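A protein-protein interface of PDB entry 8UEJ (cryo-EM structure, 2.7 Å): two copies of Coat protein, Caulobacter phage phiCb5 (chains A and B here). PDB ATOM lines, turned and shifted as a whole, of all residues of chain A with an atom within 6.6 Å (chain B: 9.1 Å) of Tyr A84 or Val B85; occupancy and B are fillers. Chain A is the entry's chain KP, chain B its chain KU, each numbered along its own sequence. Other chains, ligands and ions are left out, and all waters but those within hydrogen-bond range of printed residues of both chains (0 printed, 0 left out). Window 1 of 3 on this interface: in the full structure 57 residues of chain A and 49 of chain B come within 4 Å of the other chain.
OE1 of Gln A82 lies within hydrogen-bond range of NH1 of Arg B88. The backbone carbonyl oxygen of Tyr A84 is in hydrogen-bond range of the backbone NH of Val B86 (3.1 Å). The backbone NH (N) of Val A86 sits at hydrogen-bond distance from the backbone carbonyl oxygen (O) of Tyr B84. O of Leu A109 is in hydrogen-bond range of OG of Ser B106 (3.5 Å). O of Gly B102 is in hydrogen-bond range of OH of Tyr A114 (3.1 Å).
The backbone carbonyl oxygen of Val A85 sits close to the side-chain amide oxygen of Asn A63 (2.9 Å). The backbone NH (N) of Phe A66 is in hydrogen-bond range of the backbone carbonyl oxygen (O) of Ala A83 (2.8 Å). The backbone NH of Ile B87 is in hydrogen-bond range of the backbone carbonyl oxygen of His B62. OD1 of Asn B63 lies close to O of Val B85, at 3.1 Å. The backbone carbonyl oxygen of Val B64 sits at hydrogen-bond distance from the backbone NH of Val B85, at 2.8 Å. The backbone carbonyl oxygen (O) of Phe B66 sits at hydrogen-bond distance from the backbone NH (N) of Ala B83.
Among the printed residues, merely in contact across the chains: Tyr A84 with Val B85, Val A85 with Tyr B84, Tyr A114 with Ile B87, Val A86 with Ala B83, Leu A105 with Ala B83, Ala A83 with Leu B105, Ala A83 with Val B86, Gln A82 with Ile B87, Tyr A114 with Ser B106, Tyr A84 with Leu B105, Val A85 with Leu B109, Leu A105 with Phe B66, Leu A105 with Tyr B84 and Leu A109 with Val B85.
Of the printed residues of chain B, Tyr A84 touches Val B85 (3.3 Å), Val B86 (3.1 Å) and Leu B105 (3.9 Å). Of the printed residues of chain A, Val B85 touches Tyr A84 and Leu A109. Of chain B, only Val B86 and Leu B105 come within 4 Å of Ala A83. Of the printed residues of chain A, Phe B66 touches Leu A105 (3.9 Å). Of the printed residues of chain A, Leu B109 touches Val A85 (3.9 Å). Of the printed residues of chain B, Leu A109 touches Val B85 (3.99 Å) and Ser B106 (3.5 Å). Of the printed residues of chain A, Gly B102 touches Tyr A114 (3.1 Å). Leu B101 touches none of the printed residues of chain A.
Printed residues of chain B that touch a printed residue of chain A: Phe B66, Ala B83, Tyr B84, Val B85, Val B86, Ile B87, Arg B88, Gly B102, Leu B105, Ser B106 and Leu B109. Hydrophobic or aromatic side chains of chain B that line the printed part of chain A: Phe B66, Ala B83, Tyr B84, Val B85, Val B86, Ile B87, Leu B105 and Leu B109. Of the 12 printed residues of chain A, 8 touch a printed residue of chain B. Hydrophobic or aromatic side chains of chain A within 4 Å of the printed part of chain B: Ala A83, Tyr A84, Val A85, Val A86, Leu A105, Leu A109 and Tyr A114. Among the printed residues, 19 pairs touch across the chains. Among the printed residues, no Asp or Glu carboxylate lies within 4 Å of a Lys or Arg side-chain nitrogen of the other chain.
Ala A83 touches Val B86, and with the chains exchanged Val A86 touches Ala B83. Tyr A84 touches Val B85, and with the chains exchanged Val A85 touches Tyr B84. Tyr A84 touches Val B86, and with the chains exchanged Val A86 touches Tyr B84. Leu A105 touches Phe B66, but with the chains exchanged Phe A66 does not touch Leu B105 (4.3 Å). Positions printed for both chains: 63, 64, 65, 66, 82, 83, 84, 85, 86, 105, 109 and 114. Of the 19 pairs that touch across the chains among the printed residues, 12 have their exchanged pair printed and touching as well.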
ATOM      1  N   ASN A  63       9.558  18.274   7.606  1.00  0.00           N
ATOM      2  CA  ASN A  63      10.026  19.477   8.282  1.00  0.00           C
ATOM      3  C   ASN A  63       9.277  19.665   9.594  1.00  0.00           C
ATOM      4  O   ASN A  63       8.066  19.437   9.668  1.00  0.00           O
ATOM      5  CB  ASN A  63       9.841  20.706   7.381  1.00  0.00           C
ATOM      6  CG  ASN A  63      10.299  21.992   8.039  1.00  0.00           C
ATOM      7  OD1 ASN A  63      10.782  21.986   9.171  1.00  0.00           O
ATOM      8  ND2 ASN A  63      10.180  23.102   7.317  1.00  0.00           N
ATOM      9  N   VAL A  64      10.010  20.062  10.631  1.00  0.00           N
ATOM     10  CA  VAL A  64       9.450  20.347  11.947  1.00  0.00           C
ATOM     11  C   VAL A  64      10.132  21.589  12.503  1.00  0.00           C
ATOM     12  O   VAL A  64      11.353  21.744  12.372  1.00  0.00           O
ATOM     13  CB  VAL A  64       9.623  19.150  12.905  1.00  0.00           C
ATOM     14  CG1 VAL A  64       9.101  19.493  14.295  1.00  0.00           C
ATOM     15  CG2 VAL A  64       8.912  17.927  12.344  1.00  0.00           C
ATOM     16  N   GLU A  65       9.352  22.475  13.125  1.00  0.00           N
ATOM     17  CA  GLU A  65       9.878  23.743  13.612  1.00  0.00           C
ATOM     18  C   GLU A  65       9.199  24.140  14.915  1.00  0.00           C
ATOM     19  O   GLU A  65       8.018  23.861  15.134  1.00  0.00           O
ATOM     20  CB  GLU A  65       9.694  24.872  12.584  1.00  0.00           C
ATOM     21  CG  GLU A  65       8.254  25.185  12.223  1.00  0.00           C
ATOM     22  CD  GLU A  65       7.609  26.163  13.185  1.00  0.00           C
ATOM     23  OE1 GLU A  65       8.346  26.879  13.896  1.00  0.00           O
ATOM     24  OE2 GLU A  65       6.364  26.211  13.239  1.00  0.00           O
ATOM     25  N   PHE A  66       9.968  24.806  15.773  1.00  0.00           N
ATOM     26  CA  PHE A  66       9.476  25.434  16.990  1.00  0.00           C
ATOM     27  C   PHE A  66       9.686  26.938  16.886  1.00  0.00           C
ATOM     28  O   PHE A  66      10.701  27.392  16.347  1.00  0.00           O
ATOM     29  CB  PHE A  66      10.208  24.903  18.227  1.00  0.00           C
ATOM     30  CG  PHE A  66       9.770  23.531  18.666  1.00  0.00           C
ATOM     31  CD1 PHE A  66       8.851  22.802  17.935  1.00  0.00           C
ATOM     32  CD2 PHE A  66      10.287  22.968  19.817  1.00  0.00           C
ATOM     33  CE1 PHE A  66       8.456  21.549  18.349  1.00  0.00           C
ATOM     34  CE2 PHE A  66       9.895  21.713  20.226  1.00  0.00           C
ATOM     35  CZ  PHE A  66       8.980  21.007  19.494  1.00  0.00           C
ATOM     36  N   GLN A  82      13.286  30.982  16.908  1.00  0.00           N
ATOM     37  CA  GLN A  82      12.834  29.916  16.025  1.00  0.00           C
ATOM     38  C   GLN A  82      13.942  28.886  15.869  1.00  0.00           C
ATOM     39  O   GLN A  82      15.128  29.208  15.971  1.00  0.00           O
ATOM     40  CB  GLN A  82      12.419  30.498  14.661  1.00  0.00           C
ATOM     41  CG  GLN A  82      12.336  29.509  13.515  1.00  0.00           C
ATOM     42  CD  GLN A  82      11.842  30.159  12.235  1.00  0.00           C
ATOM     43  OE1 GLN A  82      11.540  31.353  12.213  1.00  0.00           O
ATOM     44  NE2 GLN A  82      11.765  29.382  11.163  1.00  0.00           N
ATOM     45  N   ALA A  83      13.545  27.637  15.622  1.00  0.00           N
ATOM     46  CA  ALA A  83      14.499  26.552  15.421  1.00  0.00           C
ATOM     47  C   ALA A  83      13.774  25.382  14.773  1.00  0.00           C
ATOM     48  O   ALA A  83      12.742  24.939  15.284  1.00  0.00           O
ATOM     49  CB  ALA A  83      15.130  26.124  16.748  1.00  0.00           C
ATOM     50  N   TYR A  84      14.324  24.869  13.671  1.00  0.00           N
ATOM     51  CA  TYR A  84      13.612  23.886  12.865  1.00  0.00           C
ATOM     52  C   TYR A  84      14.581  22.865  12.288  1.00  0.00           C
ATOM     53  O   TYR A  84      15.783  23.111  12.175  1.00  0.00           O
ATOM     54  CB  TYR A  84      12.822  24.566  11.740  1.00  0.00           C
ATOM     55  CG  TYR A  84      13.653  25.306  10.718  1.00  0.00           C
ATOM     56  CD1 TYR A  84      14.167  24.649   9.611  1.00  0.00           C
ATOM     57  CD2 TYR A  84      13.881  26.670  10.829  1.00  0.00           C
ATOM     58  CE1 TYR A  84      14.916  25.320   8.670  1.00  0.00           C
ATOM     59  CE2 TYR A  84      14.627  27.352   9.881  1.00  0.00           C
ATOM     60  CZ  TYR A  84      15.139  26.670   8.799  1.00  0.00           C
ATOM     61  OH  TYR A  84      15.892  27.310   7.837  1.00  0.00           O
ATOM     62  N   VAL A  85      14.031  21.708  11.911  1.00  0.00           N
ATOM     63  CA  VAL A  85      14.795  20.610  11.330  1.00  0.00           C
ATOM     64  C   VAL A  85      14.085  20.123  10.074  1.00  0.00           C
ATOM     65  O   VAL A  85      12.856  20.175   9.972  1.00  0.00           O
ATOM     66  CB  VAL A  85      14.985  19.444  12.324  1.00  0.00           C
ATOM     67  CG1 VAL A  85      13.641  18.918  12.804  1.00  0.00           C
ATOM     68  CG2 VAL A  85      15.801  18.331  11.691  1.00  0.00           C
ATOM     69  N   VAL A  86      14.876  19.649   9.113  1.00  0.00           N
ATOM     70  CA  VAL A  86      14.382  19.165   7.830  1.00  0.00           C
ATOM     71  C   VAL A  86      15.090  17.864   7.491  1.00  0.00           C
ATOM     72  O   VAL A  86      16.297  17.727   7.716  1.00  0.00           O
ATOM     73  CB  VAL A  86      14.611  20.202   6.715  1.00  0.00           C
ATOM     74  CG1 VAL A  86      14.127  19.672   5.371  1.00  0.00           C
ATOM     75  CG2 VAL A  86      13.931  21.521   7.060  1.00  0.00           C
ATOM     76  N   LEU A 105      22.291  13.170  14.194  1.00  0.00           N
ATOM     77  CA  LEU A 105      22.280  14.624  14.325  1.00  0.00           C
ATOM     78  C   LEU A 105      21.668  15.046  15.652  1.00  0.00           C
ATOM     79  O   LEU A 105      22.197  15.928  16.339  1.00  0.00           O
ATOM     80  CB  LEU A 105      21.509  15.239  13.154  1.00  0.00           C
ATOM     81  CG  LEU A 105      21.167  16.731  13.186  1.00  0.00           C
ATOM     82  CD1 LEU A 105      22.370  17.580  13.552  1.00  0.00           C
ATOM     83  CD2 LEU A 105      20.597  17.164  11.837  1.00  0.00           C
ATOM     84  N   LEU A 109      23.779  17.184  18.764  1.00  0.00           N
ATOM     85  CA  LEU A 109      23.414  18.491  19.294  1.00  0.00           C
ATOM     86  C   LEU A 109      23.246  18.414  20.808  1.00  0.00           C
ATOM     87  O   LEU A 109      22.570  17.524  21.331  1.00  0.00           O
ATOM     88  CB  LEU A 109      22.123  18.980  18.636  1.00  0.00           C
ATOM     89  CG  LEU A 109      22.183  19.226  17.124  1.00  0.00           C
ATOM     90  CD1 LEU A 109      20.804  19.565  16.572  1.00  0.00           C
ATOM     91  CD2 LEU A 109      23.176  20.326  16.774  1.00  0.00           C
ATOM     92  N   TYR A 114      25.464  24.165  21.210  1.00  0.00           N
ATOM     93  CA  TYR A 114      24.651  25.351  20.970  1.00  0.00           C
ATOM     94  C   TYR A 114      25.390  26.613  21.391  1.00  0.00           C
ATOM     95  O   TYR A 114      25.352  27.629  20.685  1.00  0.00           O
ATOM     96  CB  TYR A 114      23.306  25.230  21.683  1.00  0.00           C
ATOM     97  CG  TYR A 114      22.352  24.282  20.994  1.00  0.00           C
ATOM     98  CD1 TYR A 114      21.580  24.713  19.925  1.00  0.00           C
ATOM     99  CD2 TYR A 114      22.226  22.963  21.398  1.00  0.00           C
ATOM    100  CE1 TYR A 114      20.709  23.859  19.287  1.00  0.00           C
ATOM    101  CE2 TYR A 114      21.355  22.102  20.762  1.00  0.00           C
ATOM    102  CZ  TYR A 114      20.601  22.555  19.709  1.00  0.00           C
ATOM    103  OH  TYR A 114      19.729  21.705  19.067  1.00  0.00           O
ATOM    104  N   LYS B  44      28.946  20.287   6.862  1.00  0.00           N
ATOM    105  CA  LYS B  44      29.250  21.699   6.680  1.00  0.00           C
ATOM    106  C   LYS B  44      28.603  22.498   7.801  1.00  0.00           C
ATOM    107  O   LYS B  44      27.605  22.073   8.389  1.00  0.00           O
ATOM    108  CB  LYS B  44      28.756  22.224   5.322  1.00  0.00           C
ATOM    109  CG  LYS B  44      29.023  21.291   4.150  1.00  0.00           C
ATOM    110  CD  LYS B  44      28.598  21.902   2.815  1.00  0.00           C
ATOM    111  CE  LYS B  44      29.375  23.155   2.444  1.00  0.00           C
ATOM    112  NZ  LYS B  44      29.583  23.236   0.968  1.00  0.00           N
ATOM    113  N   VAL B  45      29.192  23.653   8.105  1.00  0.00           N
ATOM    114  CA  VAL B  45      28.634  24.607   9.057  1.00  0.00           C
ATOM    115  C   VAL B  45      28.626  25.977   8.396  1.00  0.00           C
ATOM    116  O   VAL B  45      29.571  26.336   7.685  1.00  0.00           O
ATOM    117  CB  VAL B  45      29.432  24.643  10.376  1.00  0.00           C
ATOM    118  CG1 VAL B  45      28.893  25.735  11.289  1.00  0.00           C
ATOM    119  CG2 VAL B  45      29.383  23.290  11.064  1.00  0.00           C
ATOM    120  N   ARG B  46      27.555  26.738   8.620  1.00  0.00           N
ATOM    121  CA  ARG B  46      27.379  28.037   7.988  1.00  0.00           C
ATOM    122  C   ARG B  46      26.800  29.032   8.985  1.00  0.00           C
ATOM    123  O   ARG B  46      26.018  28.670   9.867  1.00  0.00           O
ATOM    124  CB  ARG B  46      26.463  27.936   6.755  1.00  0.00           C
ATOM    125  CG  ARG B  46      26.339  29.238   5.970  1.00  0.00           C
ATOM    126  CD  ARG B  46      25.514  29.089   4.690  1.00  0.00           C
ATOM    127  NE  ARG B  46      26.060  28.104   3.761  1.00  0.00           N
ATOM    128  CZ  ARG B  46      25.717  26.823   3.722  1.00  0.00           C
ATOM    129  NH1 ARG B  46      24.841  26.311   4.576  1.00  0.00           N
ATOM    130  NH2 ARG B  46      26.266  26.034   2.802  1.00  0.00           N
ATOM    131  N   GLU B  60      19.984  36.629  13.231  1.00  0.00           N
ATOM    132  CA  GLU B  60      21.155  35.806  12.969  1.00  0.00           C
ATOM    133  C   GLU B  60      20.715  34.369  12.722  1.00  0.00           C
ATOM    134  O   GLU B  60      19.876  33.840  13.456  1.00  0.00           O
ATOM    135  CB  GLU B  60      22.130  35.885  14.151  1.00  0.00           C
ATOM    136  CG  GLU B  60      23.424  35.127  13.972  1.00  0.00           C
ATOM    137  CD  GLU B  60      24.348  35.304  15.161  1.00  0.00           C
ATOM    138  OE1 GLU B  60      23.958  36.004  16.118  1.00  0.00           O
ATOM    139  OE2 GLU B  60      25.460  34.739  15.140  1.00  0.00           O
ATOM    140  N   ARG B  61      21.290  33.736  11.697  1.00  0.00           N
ATOM    141  CA  ARG B  61      20.950  32.367  11.317  1.00  0.00           C
ATOM    142  C   ARG B  61      22.186  31.484  11.389  1.00  0.00           C
ATOM    143  O   ARG B  61      23.248  31.849  10.876  1.00  0.00           O
ATOM    144  CB  ARG B  61      20.366  32.291   9.889  1.00  0.00           C
ATOM    145  CG  ARG B  61      19.073  33.067   9.654  1.00  0.00           C
ATOM    146  CD  ARG B  61      18.869  33.343   8.161  1.00  0.00           C
ATOM    147  NE  ARG B  61      17.812  34.316   7.899  1.00  0.00           N
ATOM    148  CZ  ARG B  61      16.565  34.007   7.560  1.00  0.00           C
ATOM    149  NH1 ARG B  61      16.168  32.747   7.428  1.00  0.00           N
ATOM    150  NH2 ARG B  61      15.691  34.988   7.339  1.00  0.00           N
ATOM    151  N   HIS B  62      22.035  30.311  12.007  1.00  0.00           N
ATOM    152  CA  HIS B  62      23.119  29.355  12.190  1.00  0.00           C
ATOM    153  C   HIS B  62      22.653  27.996  11.687  1.00  0.00           C
ATOM    154  O   HIS B  62      21.577  27.532  12.078  1.00  0.00           O
ATOM    155  CB  HIS B  62      23.518  29.274  13.665  1.00  0.00           C
ATOM    156  CG  HIS B  62      24.159  30.524  14.183  1.00  0.00           C
ATOM    157  ND1 HIS B  62      24.424  30.727  15.519  1.00  0.00           N
ATOM    158  CD2 HIS B  62      24.587  31.638  13.543  1.00  0.00           C
ATOM    159  CE1 HIS B  62      24.986  31.911  15.681  1.00  0.00           C
ATOM    160  NE2 HIS B  62      25.100  32.483  14.496  1.00  0.00           N
ATOM    161  N   ASN B  63      23.455  27.352  10.832  1.00  0.00           N
ATOM    162  CA  ASN B  63      23.015  26.177  10.087  1.00  0.00           C
ATOM    163  C   ASN B  63      24.033  25.051  10.207  1.00  0.00           C
ATOM    164  O   ASN B  63      25.244  25.290  10.179  1.00  0.00           O
ATOM    165  CB  ASN B  63      22.796  26.526   8.606  1.00  0.00           C
ATOM    166  CG  ASN B  63      22.399  25.322   7.769  1.00  0.00           C
ATOM    167  OD1 ASN B  63      22.288  24.206   8.274  1.00  0.00           O
ATOM    168  ND2 ASN B  63      22.179  25.549   6.478  1.00  0.00           N
ATOM    169  N   VAL B  64      23.533  23.822  10.341  1.00  0.00           N
ATOM    170  CA  VAL B  64      24.356  22.617  10.393  1.00  0.00           C
ATOM    171  C   VAL B  64      23.637  21.490   9.661  1.00  0.00           C
ATOM    172  O   VAL B  64      22.435  21.282   9.863  1.00  0.00           O
ATOM    173  CB  VAL B  64      24.662  22.216  11.848  1.00  0.00           C
ATOM    174  CG1 VAL B  64      25.389  20.879  11.899  1.00  0.00           C
ATOM    175  CG2 VAL B  64      25.487  23.301  12.513  1.00  0.00           C
ATOM    176  N   GLU B  65      24.370  20.755   8.821  1.00  0.00           N
ATOM    177  CA  GLU B  65      23.771  19.701   8.012  1.00  0.00           C
ATOM    178  C   GLU B  65      24.748  18.546   7.832  1.00  0.00           C
ATOM    179  O   GLU B  65      25.961  18.746   7.727  1.00  0.00           O
ATOM    180  CB  GLU B  65      23.332  20.227   6.632  1.00  0.00           C
ATOM    181  CG  GLU B  65      24.434  20.775   5.745  1.00  0.00           C
ATOM    182  CD  GLU B  65      25.116  19.694   4.932  1.00  0.00           C
ATOM    183  OE1 GLU B  65      24.521  18.609   4.761  1.00  0.00           O
ATOM    184  OE2 GLU B  65      26.246  19.932   4.456  1.00  0.00           O
ATOM    185  N   PHE B  66      24.196  17.335   7.791  1.00  0.00           N
ATOM    186  CA  PHE B  66      24.916  16.119   7.433  1.00  0.00           C
ATOM    187  C   PHE B  66      24.400  15.596   6.101  1.00  0.00           C
ATOM    188  O   PHE B  66      23.203  15.665   5.819  1.00  0.00           O
ATOM    189  CB  PHE B  66      24.742  15.029   8.495  1.00  0.00           C
ATOM    190  CG  PHE B  66      25.329  15.374   9.831  1.00  0.00           C
ATOM    191  CD1 PHE B  66      26.164  16.464   9.978  1.00  0.00           C
ATOM    192  CD2 PHE B  66      25.035  14.611  10.943  1.00  0.00           C
ATOM    193  CE1 PHE B  66      26.704  16.774  11.201  1.00  0.00           C
ATOM    194  CE2 PHE B  66      25.570  14.928  12.170  1.00  0.00           C
ATOM    195  CZ  PHE B  66      26.404  16.006  12.297  1.00  0.00           C
ATOM    196  N   GLN B  82      20.410  13.398   3.593  1.00  0.00           N
ATOM    197  CA  GLN B  82      20.893  14.453   4.470  1.00  0.00           C
ATOM    198  C   GLN B  82      19.762  14.953   5.359  1.00  0.00           C
ATOM    199  O   GLN B  82      18.582  14.855   5.016  1.00  0.00           O
ATOM    200  CB  GLN B  82      21.481  15.625   3.667  1.00  0.00           C
ATOM    201  CG  GLN B  82      20.529  16.228   2.636  1.00  0.00           C
ATOM    202  CD  GLN B  82      21.148  17.366   1.852  1.00  0.00           C
ATOM    203  OE1 GLN B  82      21.129  17.363   0.622  1.00  0.00           O
ATOM    204  NE2 GLN B  82      21.711  18.341   2.560  1.00  0.00           N
ATOM    205  N   ALA B  83      20.151  15.522   6.500  1.00  0.00           N
ATOM    206  CA  ALA B  83      19.227  16.104   7.465  1.00  0.00           C
ATOM    207  C   ALA B  83      19.940  17.261   8.149  1.00  0.00           C
ATOM    208  O   ALA B  83      21.110  17.136   8.516  1.00  0.00           O
ATOM    209  CB  ALA B  83      18.769  15.076   8.505  1.00  0.00           C
ATOM    210  N   TYR B  84      19.236  18.377   8.333  1.00  0.00           N
ATOM    211  CA  TYR B  84      19.895  19.605   8.751  1.00  0.00           C
ATOM    212  C   TYR B  84      19.021  20.360   9.741  1.00  0.00           C
ATOM    213  O   TYR B  84      17.811  20.139   9.827  1.00  0.00           O
ATOM    214  CB  TYR B  84      20.232  20.498   7.548  1.00  0.00           C
ATOM    215  CG  TYR B  84      19.061  20.984   6.723  1.00  0.00           C
ATOM    216  CD1 TYR B  84      18.600  20.259   5.635  1.00  0.00           C
ATOM    217  CD2 TYR B  84      18.444  22.190   7.009  1.00  0.00           C
ATOM    218  CE1 TYR B  84      17.542  20.710   4.872  1.00  0.00           C
ATOM    219  CE2 TYR B  84      17.383  22.650   6.247  1.00  0.00           C
ATOM    220  CZ  TYR B  84      16.940  21.909   5.173  1.00  0.00           C
ATOM    221  OH  TYR B  84      15.880  22.331   4.396  1.00  0.00           O
ATOM    222  N   VAL B  85      19.659  21.256  10.494  1.00  0.00           N
ATOM    223  CA  VAL B  85      18.979  22.086  11.480  1.00  0.00           C
ATOM    224  C   VAL B  85      19.403  23.535  11.290  1.00  0.00           C
ATOM    225  O   VAL B  85      20.494  23.823  10.789  1.00  0.00           O
ATOM    226  CB  VAL B  85      19.272  21.633  12.925  1.00  0.00           C
ATOM    227  CG1 VAL B  85      20.758  21.727  13.223  1.00  0.00           C
ATOM    228  CG2 VAL B  85      18.483  22.475  13.912  1.00  0.00           C
ATOM    229  N   VAL B  86      18.524  24.451  11.692  1.00  0.00           N
ATOM    230  CA  VAL B  86      18.770  25.886  11.612  1.00  0.00           C
ATOM    231  C   VAL B  86      18.255  26.540  12.885  1.00  0.00           C
ATOM    232  O   VAL B  86      17.264  26.092  13.469  1.00  0.00           O
ATOM    233  CB  VAL B  86      18.099  26.510  10.374  1.00  0.00           C
ATOM    234  CG1 VAL B  86      18.638  27.905  10.121  1.00  0.00           C
ATOM    235  CG2 VAL B  86      18.297  25.622   9.151  1.00  0.00           C
ATOM    236  N   ILE B  87      18.935  27.599  13.318  1.00  0.00           N
ATOM    237  CA  ILE B  87      18.540  28.386  14.480  1.00  0.00           C
ATOM    238  C   ILE B  87      18.517  29.855  14.086  1.00  0.00           C
ATOM    239  O   ILE B  87      19.385  30.314  13.337  1.00  0.00           O
ATOM    240  CB  ILE B  87      19.493  28.161  15.668  1.00  0.00           C
ATOM    241  CG1 ILE B  87      19.437  26.704  16.117  1.00  0.00           C
ATOM    242  CG2 ILE B  87      19.140  29.095  16.804  1.00  0.00           C
ATOM    243  CD1 ILE B  87      20.516  26.331  17.097  1.00  0.00           C
ATOM    244  N   ARG B  88      17.529  30.593  14.593  1.00  0.00           N
ATOM    245  CA  ARG B  88      17.360  31.995  14.231  1.00  0.00           C
ATOM    246  C   ARG B  88      17.024  32.801  15.476  1.00  0.00           C
ATOM    247  O   ARG B  88      16.109  32.442  16.223  1.00  0.00           O
ATOM    248  CB  ARG B  88      16.277  32.135  13.146  1.00  0.00           C
ATOM    249  CG  ARG B  88      15.836  33.550  12.785  1.00  0.00           C
ATOM    250  CD  ARG B  88      15.154  33.552  11.409  1.00  0.00           C
ATOM    251  NE  ARG B  88      14.202  34.634  11.184  1.00  0.00           N
ATOM    252  CZ  ARG B  88      13.115  34.850  11.912  1.00  0.00           C
ATOM    253  NH1 ARG B  88      12.754  34.023  12.881  1.00  0.00           N
ATOM    254  NH2 ARG B  88      12.358  35.910  11.645  1.00  0.00           N
ATOM    255  N   LEU B 101      15.921  26.643  24.051  1.00  0.00           N
ATOM    256  CA  LEU B 101      15.032  26.217  22.974  1.00  0.00           C
ATOM    257  C   LEU B 101      15.686  25.130  22.126  1.00  0.00           C
ATOM    258  O   LEU B 101      15.024  24.171  21.702  1.00  0.00           O
ATOM    259  CB  LEU B 101      14.651  27.423  22.111  1.00  0.00           C
ATOM    260  CG  LEU B 101      13.555  27.231  21.061  1.00  0.00           C
ATOM    261  CD1 LEU B 101      12.181  27.248  21.702  1.00  0.00           C
ATOM    262  CD2 LEU B 101      13.658  28.304  19.979  1.00  0.00           C
ATOM    263  N   GLY B 102      16.988  25.264  21.863  1.00  0.00           N
ATOM    264  CA  GLY B 102      17.682  24.251  21.087  1.00  0.00           C
ATOM    265  C   GLY B 102      17.682  22.891  21.760  1.00  0.00           C
ATOM    266  O   GLY B 102      17.436  21.870  21.114  1.00  0.00           O
ATOM    267  N   LEU B 105      14.249  21.317  21.386  1.00  0.00           N
ATOM    268  CA  LEU B 105      14.023  20.693  20.085  1.00  0.00           C
ATOM    269  C   LEU B 105      14.812  19.399  19.951  1.00  0.00           C
ATOM    270  O   LEU B 105      14.294  18.397  19.442  1.00  0.00           O
ATOM    271  CB  LEU B 105      14.395  21.665  18.963  1.00  0.00           C
ATOM    272  CG  LEU B 105      14.280  21.153  17.522  1.00  0.00           C
ATOM    273  CD1 LEU B 105      12.931  20.507  17.274  1.00  0.00           C
ATOM    274  CD2 LEU B 105      14.508  22.297  16.536  1.00  0.00           C
ATOM    275  N   SER B 106      16.069  19.399  20.397  1.00  0.00           N
ATOM    276  CA  SER B 106      16.896  18.204  20.270  1.00  0.00           C
ATOM    277  C   SER B 106      16.341  17.053  21.103  1.00  0.00           C
ATOM    278  O   SER B 106      16.319  15.903  20.651  1.00  0.00           O
ATOM    279  CB  SER B 106      18.333  18.525  20.682  1.00  0.00           C
ATOM    280  OG  SER B 106      19.157  17.379  20.598  1.00  0.00           O
ATOM    281  N   LEU B 109      13.030  15.236  19.474  1.00  0.00           N
ATOM    282  CA  LEU B 109      13.201  14.254  18.412  1.00  0.00           C
ATOM    283  C   LEU B 109      13.835  12.976  18.953  1.00  0.00           C
ATOM    284  O   LEU B 109      14.666  13.000  19.863  1.00  0.00           O
ATOM    285  CB  LEU B 109      14.060  14.828  17.283  1.00  0.00           C
ATOM    286  CG  LEU B 109      13.696  16.224  16.776  1.00  0.00           C
ATOM    287  CD1 LEU B 109      14.757  16.746  15.818  1.00  0.00           C
ATOM    288  CD2 LEU B 109      12.333  16.207  16.106  1.00  0.00           C
ATOM    289  N   TYR B 114      10.813   9.835  14.604  1.00  0.00           N
ATOM    290  CA  TYR B 114      11.307   9.749  13.237  1.00  0.00           C
ATOM    291  C   TYR B 114      10.537   8.692  12.453  1.00  0.00           C
ATOM    292  O   TYR B 114      10.210   8.892  11.275  1.00  0.00           O
ATOM    293  CB  TYR B 114      12.809   9.462  13.259  1.00  0.00           C
ATOM    294  CG  TYR B 114      13.679  10.683  13.524  1.00  0.00           C
ATOM    295  CD1 TYR B 114      13.253  11.967  13.195  1.00  0.00           C
ATOM    296  CD2 TYR B 114      14.909  10.553  14.152  1.00  0.00           C
ATOM    297  CE1 TYR B 114      14.046  13.069  13.449  1.00  0.00           C
ATOM    298  CE2 TYR B 114      15.700  11.653  14.413  1.00  0.00           C
ATOM    299  CZ  TYR B 114      15.265  12.905  14.061  1.00  0.00           C
ATOM    300  OH  TYR B 114      16.059  14.000  14.324  1.00  0.00           O
